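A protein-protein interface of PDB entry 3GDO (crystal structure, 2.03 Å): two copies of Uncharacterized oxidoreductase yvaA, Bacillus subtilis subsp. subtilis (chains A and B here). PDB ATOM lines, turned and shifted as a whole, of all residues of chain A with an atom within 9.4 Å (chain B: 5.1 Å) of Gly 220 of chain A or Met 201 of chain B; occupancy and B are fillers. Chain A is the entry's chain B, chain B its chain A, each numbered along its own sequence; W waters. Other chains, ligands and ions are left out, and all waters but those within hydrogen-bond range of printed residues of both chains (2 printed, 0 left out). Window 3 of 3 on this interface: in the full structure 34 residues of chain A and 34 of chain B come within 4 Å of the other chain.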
ATOM      1  N   ILE A 146      35.845  -0.603 -24.920  1.00  0.00           N
ATOM      2  CA  ILE A 146      35.568  -1.387 -23.724  1.00  0.00           C
ATOM      3  C   ILE A 146      34.280  -2.154 -23.988  1.00  0.00           C
ATOM      4  O   ILE A 146      33.301  -1.565 -24.472  1.00  0.00           O
ATOM      5  CB  ILE A 146      35.473  -0.487 -22.479  1.00  0.00           C
ATOM      6  CG1 ILE A 146      36.884  -0.008 -22.112  1.00  0.00           C
ATOM      7  CG2 ILE A 146      34.820  -1.242 -21.315  1.00  0.00           C
ATOM      8  CD1 ILE A 146      36.910   1.232 -21.157  1.00  0.00           C
ATOM      9  N   ASN A 147      34.305  -3.470 -23.734  1.00  0.00           N
ATOM     10  CA  ASN A 147      33.114  -4.284 -23.983  1.00  0.00           C
ATOM     11  C   ASN A 147      32.455  -4.770 -22.681  1.00  0.00           C
ATOM     12  O   ASN A 147      31.280  -5.100 -22.661  1.00  0.00           O
ATOM     13  CB  ASN A 147      33.435  -5.454 -24.939  1.00  0.00           C
ATOM     14  CG  ASN A 147      34.449  -6.431 -24.363  1.00  0.00           C
ATOM     15  OD1 ASN A 147      34.164  -7.149 -23.388  1.00  0.00           O
ATOM     16  ND2 ASN A 147      35.628  -6.475 -24.956  1.00  0.00           N
ATOM     17  N   THR A 148      33.237  -4.825 -21.609  1.00  0.00           N
ATOM     18  CA  THR A 148      32.749  -5.311 -20.319  1.00  0.00           C
ATOM     19  C   THR A 148      33.384  -4.475 -19.218  1.00  0.00           C
ATOM     20  O   THR A 148      34.638  -4.282 -19.187  1.00  0.00           O
ATOM     21  CB  THR A 148      33.111  -6.818 -20.092  1.00  0.00           C
ATOM     22  OG1 THR A 148      32.617  -7.604 -21.166  1.00  0.00           O
ATOM     23  CG2 THR A 148      32.480  -7.360 -18.827  1.00  0.00           C
ATOM     24  N   MET A 192      24.302   7.458 -20.423  1.00  0.00           N
ATOM     25  CA  MET A 192      23.192   6.681 -19.938  1.00  0.00           C
ATOM     26  C   MET A 192      23.077   5.382 -20.722  1.00  0.00           C
ATOM     27  O   MET A 192      23.282   5.378 -21.950  1.00  0.00           O
ATOM     28  CB  MET A 192      21.872   7.479 -20.043  1.00  0.00           C
ATOM     29  CG  MET A 192      21.654   8.562 -18.920  1.00  0.00           C
ATOM     30  SD  MET A 192      21.604   7.923 -17.211  1.00  0.00           S
ATOM     31  CE  MET A 192      19.884   7.630 -17.027  1.00  0.00           C
ATOM     32  N   PRO A 193      22.717   4.274 -20.021  1.00  0.00           N
ATOM     33  CA  PRO A 193      22.487   2.992 -20.673  1.00  0.00           C
ATOM     34  C   PRO A 193      21.094   2.940 -21.301  1.00  0.00           C
ATOM     35  O   PRO A 193      20.285   3.834 -21.104  1.00  0.00           O
ATOM     36  CB  PRO A 193      22.568   1.992 -19.506  1.00  0.00           C
ATOM     37  CG  PRO A 193      22.036   2.766 -18.335  1.00  0.00           C
ATOM     38  CD  PRO A 193      22.530   4.191 -18.553  1.00  0.00           C
ATOM     39  N   LYS A 194      20.781   1.886 -22.034  1.00  0.00           N
ATOM     40  CA  LYS A 194      19.429   1.816 -22.539  1.00  0.00           C
ATOM     41  C   LYS A 194      18.497   0.994 -21.673  1.00  0.00           C
ATOM     42  O   LYS A 194      17.286   1.057 -21.857  1.00  0.00           O
ATOM     43  CB  LYS A 194      19.369   1.393 -23.987  1.00  0.00           C
ATOM     44  CG  LYS A 194      20.187   0.214 -24.393  1.00  0.00           C
ATOM     45  CD  LYS A 194      20.164   0.193 -25.928  1.00  0.00           C
ATOM     46  CE  LYS A 194      21.095  -0.850 -26.536  1.00  0.00           C
ATOM     47  NZ  LYS A 194      20.496  -2.216 -26.436  1.00  0.00           N
ATOM     48  N   ALA A 195      19.054   0.253 -20.707  1.00  0.00           N
ATOM     49  CA  ALA A 195      18.219  -0.519 -19.817  1.00  0.00           C
ATOM     50  C   ALA A 195      18.991  -0.886 -18.565  1.00  0.00           C
ATOM     51  O   ALA A 195      20.233  -0.780 -18.541  1.00  0.00           O
ATOM     52  CB  ALA A 195      17.664  -1.754 -20.528  1.00  0.00           C
ATOM     53  N   THR A 216      22.882  -4.689 -13.826  1.00  0.00           N
ATOM     54  CA  THR A 216      23.421  -4.706 -15.177  1.00  0.00           C
ATOM     55  C   THR A 216      22.910  -3.466 -15.928  1.00  0.00           C
ATOM     56  O   THR A 216      21.670  -3.286 -16.080  1.00  0.00           O
ATOM     57  CB  THR A 216      22.996  -5.988 -15.957  1.00  0.00           C
ATOM     58  OG1 THR A 216      23.467  -7.160 -15.264  1.00  0.00           O
ATOM     59  CG2 THR A 216      23.538  -5.963 -17.398  1.00  0.00           C
ATOM     60  N   LEU A 217      23.837  -2.633 -16.367  1.00  0.00           N
ATOM     61  CA  LEU A 217      23.519  -1.496 -17.266  1.00  0.00           C
ATOM     62  C   LEU A 217      23.820  -1.832 -18.721  1.00  0.00           C
ATOM     63  O   LEU A 217      24.979  -2.111 -19.098  1.00  0.00           O
ATOM     64  CB  LEU A 217      24.226  -0.202 -16.847  1.00  0.00           C
ATOM     65  CG  LEU A 217      23.682   0.579 -15.640  1.00  0.00           C
ATOM     66  CD1 LEU A 217      23.588  -0.237 -14.363  1.00  0.00           C
ATOM     67  CD2 LEU A 217      24.544   1.836 -15.364  1.00  0.00           C
ATOM     68  N   ASP A 218      22.744  -1.833 -19.512  1.00  0.00           N
ATOM     69  CA  ASP A 218      22.775  -2.352 -20.861  1.00  0.00           C
ATOM     70  C   ASP A 218      23.173  -1.219 -21.806  1.00  0.00           C
ATOM     71  O   ASP A 218      22.409  -0.268 -22.001  1.00  0.00           O
ATOM     72  CB  ASP A 218      21.388  -2.950 -21.219  1.00  0.00           C
ATOM     73  CG  ASP A 218      21.303  -3.490 -22.674  1.00  0.00           C
ATOM     74  OD1 ASP A 218      22.330  -3.583 -23.393  1.00  0.00           O
ATOM     75  OD2 ASP A 218      20.169  -3.822 -23.091  1.00  0.00           O
ATOM     76  N   TYR A 219      24.382  -1.302 -22.339  1.00  0.00           N
ATOM     77  CA  TYR A 219      24.821  -0.381 -23.386  1.00  0.00           C
ATOM     78  C   TYR A 219      25.014  -1.159 -24.705  1.00  0.00           C
ATOM     79  O   TYR A 219      25.927  -0.865 -25.440  1.00  0.00           O
ATOM     80  CB  TYR A 219      26.149   0.246 -23.014  1.00  0.00           C
ATOM     81  CG  TYR A 219      26.153   1.160 -21.793  1.00  0.00           C
ATOM     82  CD1 TYR A 219      26.022   2.563 -21.933  1.00  0.00           C
ATOM     83  CD2 TYR A 219      26.328   0.639 -20.508  1.00  0.00           C
ATOM     84  CE1 TYR A 219      26.056   3.422 -20.809  1.00  0.00           C
ATOM     85  CE2 TYR A 219      26.383   1.484 -19.390  1.00  0.00           C
ATOM     86  CZ  TYR A 219      26.233   2.872 -19.542  1.00  0.00           C
ATOM     87  OH  TYR A 219      26.272   3.672 -18.428  1.00  0.00           O
ATOM     88  N   GLY A 220      24.205  -2.183 -24.968  1.00  0.00           N
ATOM     89  CA  GLY A 220      24.308  -2.934 -26.240  1.00  0.00           C
ATOM     90  C   GLY A 220      25.478  -3.905 -26.186  1.00  0.00           C
ATOM     91  O   GLY A 220      25.451  -4.908 -25.452  1.00  0.00           O
ATOM     92  N   LYS A 221      26.510  -3.621 -26.964  1.00  0.00           N
ATOM     93  CA  LYS A 221      27.684  -4.464 -26.983  1.00  0.00           C
ATOM     94  C   LYS A 221      28.395  -4.380 -25.615  1.00  0.00           C
ATOM     95  O   LYS A 221      28.837  -5.406 -25.068  1.00  0.00           O
ATOM     96  CB  LYS A 221      28.607  -4.040 -28.111  1.00  0.00           C
ATOM     97  CG  LYS A 221      29.855  -4.903 -28.198  1.00  0.00           C
ATOM     98  CD  LYS A 221      30.808  -4.384 -29.285  1.00  0.00           C
ATOM     99  CE  LYS A 221      32.208  -4.950 -29.052  1.00  0.00           C
ATOM    100  NZ  LYS A 221      33.169  -4.474 -30.079  1.00  0.00           N
ATOM    101  N   LEU A 222      28.481  -3.164 -25.082  1.00  0.00           N
ATOM    102  CA  LEU A 222      29.044  -2.894 -23.751  1.00  0.00           C
ATOM    103  C   LEU A 222      28.066  -3.288 -22.636  1.00  0.00           C
ATOM    104  O   LEU A 222      26.872  -2.892 -22.642  1.00  0.00           O
ATOM    105  CB  LEU A 222      29.424  -1.414 -23.608  1.00  0.00           C
ATOM    106  CG  LEU A 222      29.796  -0.851 -22.221  1.00  0.00           C
ATOM    107  CD1 LEU A 222      30.989  -1.631 -21.637  1.00  0.00           C
ATOM    108  CD2 LEU A 222      30.114   0.677 -22.248  1.00  0.00           C
ATOM    109  N   GLN A 223      28.571  -4.076 -21.678  1.00  0.00           N
ATOM    110  CA  GLN A 223      27.754  -4.461 -20.497  1.00  0.00           C
ATOM    111  C   GLN A 223      28.484  -3.985 -19.266  1.00  0.00           C
ATOM    112  O   GLN A 223      29.689  -4.265 -19.110  1.00  0.00           O
ATOM    113  CB  GLN A 223      27.506  -5.978 -20.436  1.00  0.00           C
ATOM    114  CG  GLN A 223      26.709  -6.505 -21.623  1.00  0.00           C
ATOM    115  CD  GLN A 223      25.246  -6.070 -21.554  1.00  0.00           C
ATOM    116  OE1 GLN A 223      24.598  -6.179 -20.525  1.00  0.00           O
ATOM    117  NE2 GLN A 223      24.740  -5.536 -22.658  1.00  0.00           N
ATOM    118  N   ALA A 224      27.794  -3.205 -18.443  1.00  0.00           N
ATOM    119  CA  ALA A 224      28.393  -2.637 -17.232  1.00  0.00           C
ATOM    120  C   ALA A 224      27.707  -3.365 -16.105  1.00  0.00           C
ATOM    121  O   ALA A 224      26.458  -3.413 -16.073  1.00  0.00           O
ATOM    122  CB  ALA A 224      28.148  -1.115 -17.143  1.00  0.00           C
ATOM    123  N   ILE A 225      28.499  -3.964 -15.203  1.00  0.00           N
ATOM    124  CA  ILE A 225      27.924  -4.816 -14.160  1.00  0.00           C
ATOM    125  C   ILE A 225      28.387  -4.220 -12.839  1.00  0.00           C
ATOM    126  O   ILE A 225      29.597  -4.112 -12.630  1.00  0.00           O
ATOM    127  CB  ILE A 225      28.443  -6.289 -14.234  1.00  0.00           C
ATOM    128  CG1 ILE A 225      28.236  -6.964 -15.607  1.00  0.00           C
ATOM    129  CG2 ILE A 225      27.936  -7.126 -13.012  1.00  0.00           C
ATOM    130  CD1 ILE A 225      26.866  -7.016 -16.124  1.00  0.00           C
ATOM    131  N   MET A 347      13.584  -0.669 -19.195  1.00  0.00           N
ATOM    132  CA  MET A 347      14.170   0.136 -20.270  1.00  0.00           C
ATOM    133  C   MET A 347      14.039   1.639 -19.975  1.00  0.00           C
ATOM    134  O   MET A 347      13.132   2.041 -19.262  1.00  0.00           O
ATOM    135  CB  MET A 347      13.546  -0.247 -21.623  1.00  0.00           C
ATOM    136  CG  MET A 347      14.602  -0.514 -22.697  1.00  0.00           C
ATOM    137  SD  MET A 347      14.284  -1.983 -23.722  1.00  0.00           S
ATOM    138  CE  MET A 347      15.850  -2.066 -24.615  1.00  0.00           C
ATOM    139  N   ASN B 199      21.252 -12.598 -19.486  1.00  0.00           N
ATOM    140  CA  ASN B 199      21.496 -11.945 -20.760  1.00  0.00           C
ATOM    141  C   ASN B 199      22.416 -12.820 -21.582  1.00  0.00           C
ATOM    142  O   ASN B 199      23.522 -13.194 -21.142  1.00  0.00           O
ATOM    143  CB  ASN B 199      22.126 -10.554 -20.553  1.00  0.00           C
ATOM    144  CG  ASN B 199      22.383  -9.825 -21.889  1.00  0.00           C
ATOM    145  OD1 ASN B 199      21.644 -10.016 -22.856  1.00  0.00           O
ATOM    146  ND2 ASN B 199      23.436  -9.021 -21.941  1.00  0.00           N
ATOM    147  N   VAL B 200      21.968 -13.167 -22.778  1.00  0.00           N
ATOM    148  CA  VAL B 200      22.748 -14.026 -23.619  1.00  0.00           C
ATOM    149  C   VAL B 200      22.836 -13.363 -25.002  1.00  0.00           C
ATOM    150  O   VAL B 200      21.805 -13.093 -25.596  1.00  0.00           O
ATOM    151  CB  VAL B 200      22.114 -15.437 -23.648  1.00  0.00           C
ATOM    152  CG1 VAL B 200      22.863 -16.350 -24.541  1.00  0.00           C
ATOM    153  CG2 VAL B 200      22.068 -16.069 -22.220  1.00  0.00           C
ATOM    154  N   MET B 201      24.047 -13.079 -25.491  1.00  0.00           N
ATOM    155  CA  MET B 201      24.206 -12.367 -26.769  1.00  0.00           C
ATOM    156  C   MET B 201      25.464 -12.722 -27.558  1.00  0.00           C
ATOM    157  O   MET B 201      26.270 -13.564 -27.155  1.00  0.00           O
ATOM    158  CB  MET B 201      24.121 -10.828 -26.568  1.00  0.00           C
ATOM    159  CG  MET B 201      25.330 -10.210 -25.895  1.00  0.00           C
ATOM    160  SD  MET B 201      25.082  -8.494 -25.289  1.00  0.00           S
ATOM    161  CE  MET B 201      26.775  -8.141 -24.960  1.00  0.00           C
ATOM    162  N   ALA B 202      25.606 -12.061 -28.703  1.00  0.00           N
ATOM    163  CA  ALA B 202      26.814 -12.075 -29.491  1.00  0.00           C
ATOM    164  C   ALA B 202      27.398 -10.666 -29.421  1.00  0.00           C
ATOM    165  O   ALA B 202      26.797  -9.713 -29.930  1.00  0.00           O
ATOM    166  CB  ALA B 202      26.469 -12.479 -30.924  1.00  0.00           C
ATOM    167  N   GLN B 203      28.523 -10.505 -28.727  1.00  0.00           N
ATOM    168  CA  GLN B 203      29.213  -9.235 -28.696  1.00  0.00           C
ATOM    169  C   GLN B 203      30.116  -9.016 -29.906  1.00  0.00           C
ATOM    170  O   GLN B 203      30.424  -7.873 -30.236  1.00  0.00           O
ATOM    171  CB  GLN B 203      30.126  -9.133 -27.474  1.00  0.00           C
ATOM    172  CG  GLN B 203      29.510  -8.687 -26.185  1.00  0.00           C
ATOM    173  CD  GLN B 203      30.539  -8.661 -25.057  1.00  0.00           C
ATOM    174  OE1 GLN B 203      31.445  -9.513 -24.994  1.00  0.00           O
ATOM    175  NE2 GLN B 203      30.403  -7.686 -24.159  1.00  0.00           N
ATOM    176  N   THR B 209      26.347 -16.606 -33.518  1.00  0.00           N
ATOM    177  CA  THR B 209      26.035 -17.568 -32.460  1.00  0.00           C
ATOM    178  C   THR B 209      26.382 -16.905 -31.113  1.00  0.00           C
ATOM    179  O   THR B 209      27.162 -15.938 -31.088  1.00  0.00           O
ATOM    180  CB  THR B 209      26.840 -18.894 -32.649  1.00  0.00           C
ATOM    181  OG1 THR B 209      28.232 -18.664 -32.391  1.00  0.00           O
ATOM    182  CG2 THR B 209      26.708 -19.432 -34.091  1.00  0.00           C
ATOM    183  N   VAL B 210      25.827 -17.437 -30.015  1.00  0.00           N
ATOM    184  CA  VAL B 210      26.076 -16.889 -28.684  1.00  0.00           C
ATOM    185  C   VAL B 210      27.574 -16.889 -28.322  1.00  0.00           C
ATOM    186  O   VAL B 210      28.290 -17.904 -28.467  1.00  0.00           O
ATOM    187  CB  VAL B 210      25.281 -17.650 -27.622  1.00  0.00           C
ATOM    188  CG1 VAL B 210      25.682 -17.169 -26.214  1.00  0.00           C
ATOM    189  CG2 VAL B 210      23.734 -17.530 -27.889  1.00  0.00           C
ATOM    190  N   ASP B 211      28.040 -15.761 -27.816  1.00  0.00           N
ATOM    191  CA  ASP B 211      29.448 -15.631 -27.395  1.00  0.00           C
ATOM    192  C   ASP B 211      29.690 -14.915 -26.055  1.00  0.00           C
ATOM    193  O   ASP B 211      30.846 -14.618 -25.692  1.00  0.00           O
ATOM    194  CB  ASP B 211      30.308 -15.017 -28.519  1.00  0.00           C
ATOM    195  CG  ASP B 211      30.075 -13.510 -28.709  1.00  0.00           C
ATOM    196  OD1 ASP B 211      29.737 -12.780 -27.739  1.00  0.00           O
ATOM    197  OD2 ASP B 211      30.318 -13.039 -29.845  1.00  0.00           O
ATOM    198  N   TYR B 212      28.597 -14.637 -25.343  1.00  0.00           N
ATOM    199  CA  TYR B 212      28.614 -13.924 -24.068  1.00  0.00           C
ATOM    200  C   TYR B 212      27.364 -14.384 -23.355  1.00  0.00           C
ATOM    201  O   TYR B 212      26.278 -14.467 -23.977  1.00  0.00           O
ATOM    202  CB  TYR B 212      28.530 -12.399 -24.319  1.00  0.00           C
ATOM    203  CG  TYR B 212      28.330 -11.566 -23.069  1.00  0.00           C
ATOM    204  CD1 TYR B 212      29.384 -10.882 -22.495  1.00  0.00           C
ATOM    205  CD2 TYR B 212      27.083 -11.490 -22.455  1.00  0.00           C
ATOM    206  CE1 TYR B 212      29.206 -10.120 -21.314  1.00  0.00           C
ATOM    207  CE2 TYR B 212      26.893 -10.751 -21.274  1.00  0.00           C
ATOM    208  CZ  TYR B 212      27.956 -10.050 -20.724  1.00  0.00           C
ATOM    209  OH  TYR B 212      27.758  -9.290 -19.576  1.00  0.00           O
HETATM  210  O   HOH W   1      25.146  -8.738 -19.219  1.00  0.00           O
HETATM  211  O   HOH W   2      33.823 -10.055 -23.880  1.00  0.00           O
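O of Asn 147 of chain A lies within hydrogen-bond range of NE2 of Gln 203 of chain B (3.1 Å).
The side-chain sulfur of Met 201 of chain B lies close to the backbone carbonyl oxygen of Gly 220 of chain A.
OE1 of Gln 223 of chain A sits at hydrogen-bond distance from ND2 of Asn 199 of chain B, 3.4 Å away.
NE2 of Gln 203 of chain B lies within hydrogen-bond range of O of Lys 221 of chain A (2.9 Å).
N of Gln 203 of chain B sits at hydrogen-bond distance from OD1 of Asp 211 of chain B.
The side-chain hydroxyl (OG1) of Thr 148 of chain A lies within hydrogen-bond range of the side-chain amide oxygen (OD1) of Asn 147 of chain A (2.7 Å).
N of Met 201 of chain B sits at hydrogen-bond distance from O of Tyr 212 of chain B.
The backbone NH of Gln 223 of chain A sits at hydrogen-bond distance from the backbone carbonyl oxygen of Asn 147 of chain A.
The backbone NH (N) of Asp 211 of chain B is in hydrogen-bond range of the backbone carbonyl oxygen (O) of Met 201 of chain B, 2.9 Å away.
The side-chain carboxylate (OD1) of Asp 218 of chain A sits at hydrogen-bond distance from the backbone NH (N) of Gly 220 of chain A (2.8 Å).
Gln 203 of chain B touches Thr 148 of chain A.
O of Lys 221 of chain A touches CE of Met 201 of chain B, at 3.4 Å.
Gln 223 of chain A touches Met 201 of chain B (CG to CE, 3.7 Å).
OH of Tyr 212 of chain B touches CB of Gln 223 of chain A (3.4 Å).
Of the printed residues of chain B, Asn 147 of chain A touches Gln 203.
Of the printed residues of chain B, Thr 148 of chain A touches Gln 203 (3.7 Å).
Pro 193 of chain A touches none of the printed residues of chain B.
Lys 194 of chain A touches none of the printed residues of chain B.
Gly 220 of chain A touches just one residue of chain B: Met 201 (3.5 Å).
Of the printed residues of chain B, Lys 221 of chain A touches Met 201 (3.4 Å) and Gln 203 (2.9 Å).
Printed residues of chain A within 4 Å of Asn 199 of chain B: Gln 223.
No residue of chain A comes within 4 Å of Val 200 of chain B.
Of the printed residues of chain A, Met 201 of chain B touches Gly 220 (3.5 Å), Lys 221 (3.4 Å) and Gln 223 (3.7 Å).
No residue of chain A comes within 4 Å of Ala 202 of chain B.
Of the printed residues of chain A, Gln 203 of chain B touches Asn 147 (3.1 Å), Thr 148 (3.7 Å) and Lys 221 (2.9 Å).
No residue of chain A comes within 4 Å of Val 210 of chain B.
Asp 211 of chain B touches none of the printed residues of chain A.
Printed residues of chain A that touch a printed residue of chain B: Asn 147, Thr 148, Gly 220, Lys 221 and Gln 223.
Along chain A the printed residues that touch a printed residue of chain B span positions 147 to 223.
Of the 9 printed residues of chain B, 4 touch a printed residue of chain A.
Printed residues of chain B that touch a printed residue of chain A: Asn 199, Met 201, Gln 203 and Tyr 212.
Along chain B the printed residues that touch a printed residue of chain A span positions 199 to 212.
Among the printed residues, no Asp or Glu carboxylate lies within 4 Å of a Lys or Arg side-chain nitrogen of the other chain.
No position is printed for both chains.
Of the 8 pairs that touch across the chains among the printed residues, none has its exchanged pair printed and touching as well.
Water W2 bridges OE1 of Gln 203 of chain B (2.7 Å) and OD1 of Asn 147 of chain A (3.0 Å).
Water W1 lies within hydrogen-bond range of OH of Tyr 212 of chain B (2.7 Å), OE1 of Gln 223 of chain A (2.9 Å) and ND2 of Asn 199 of chain B (3.2 Å).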
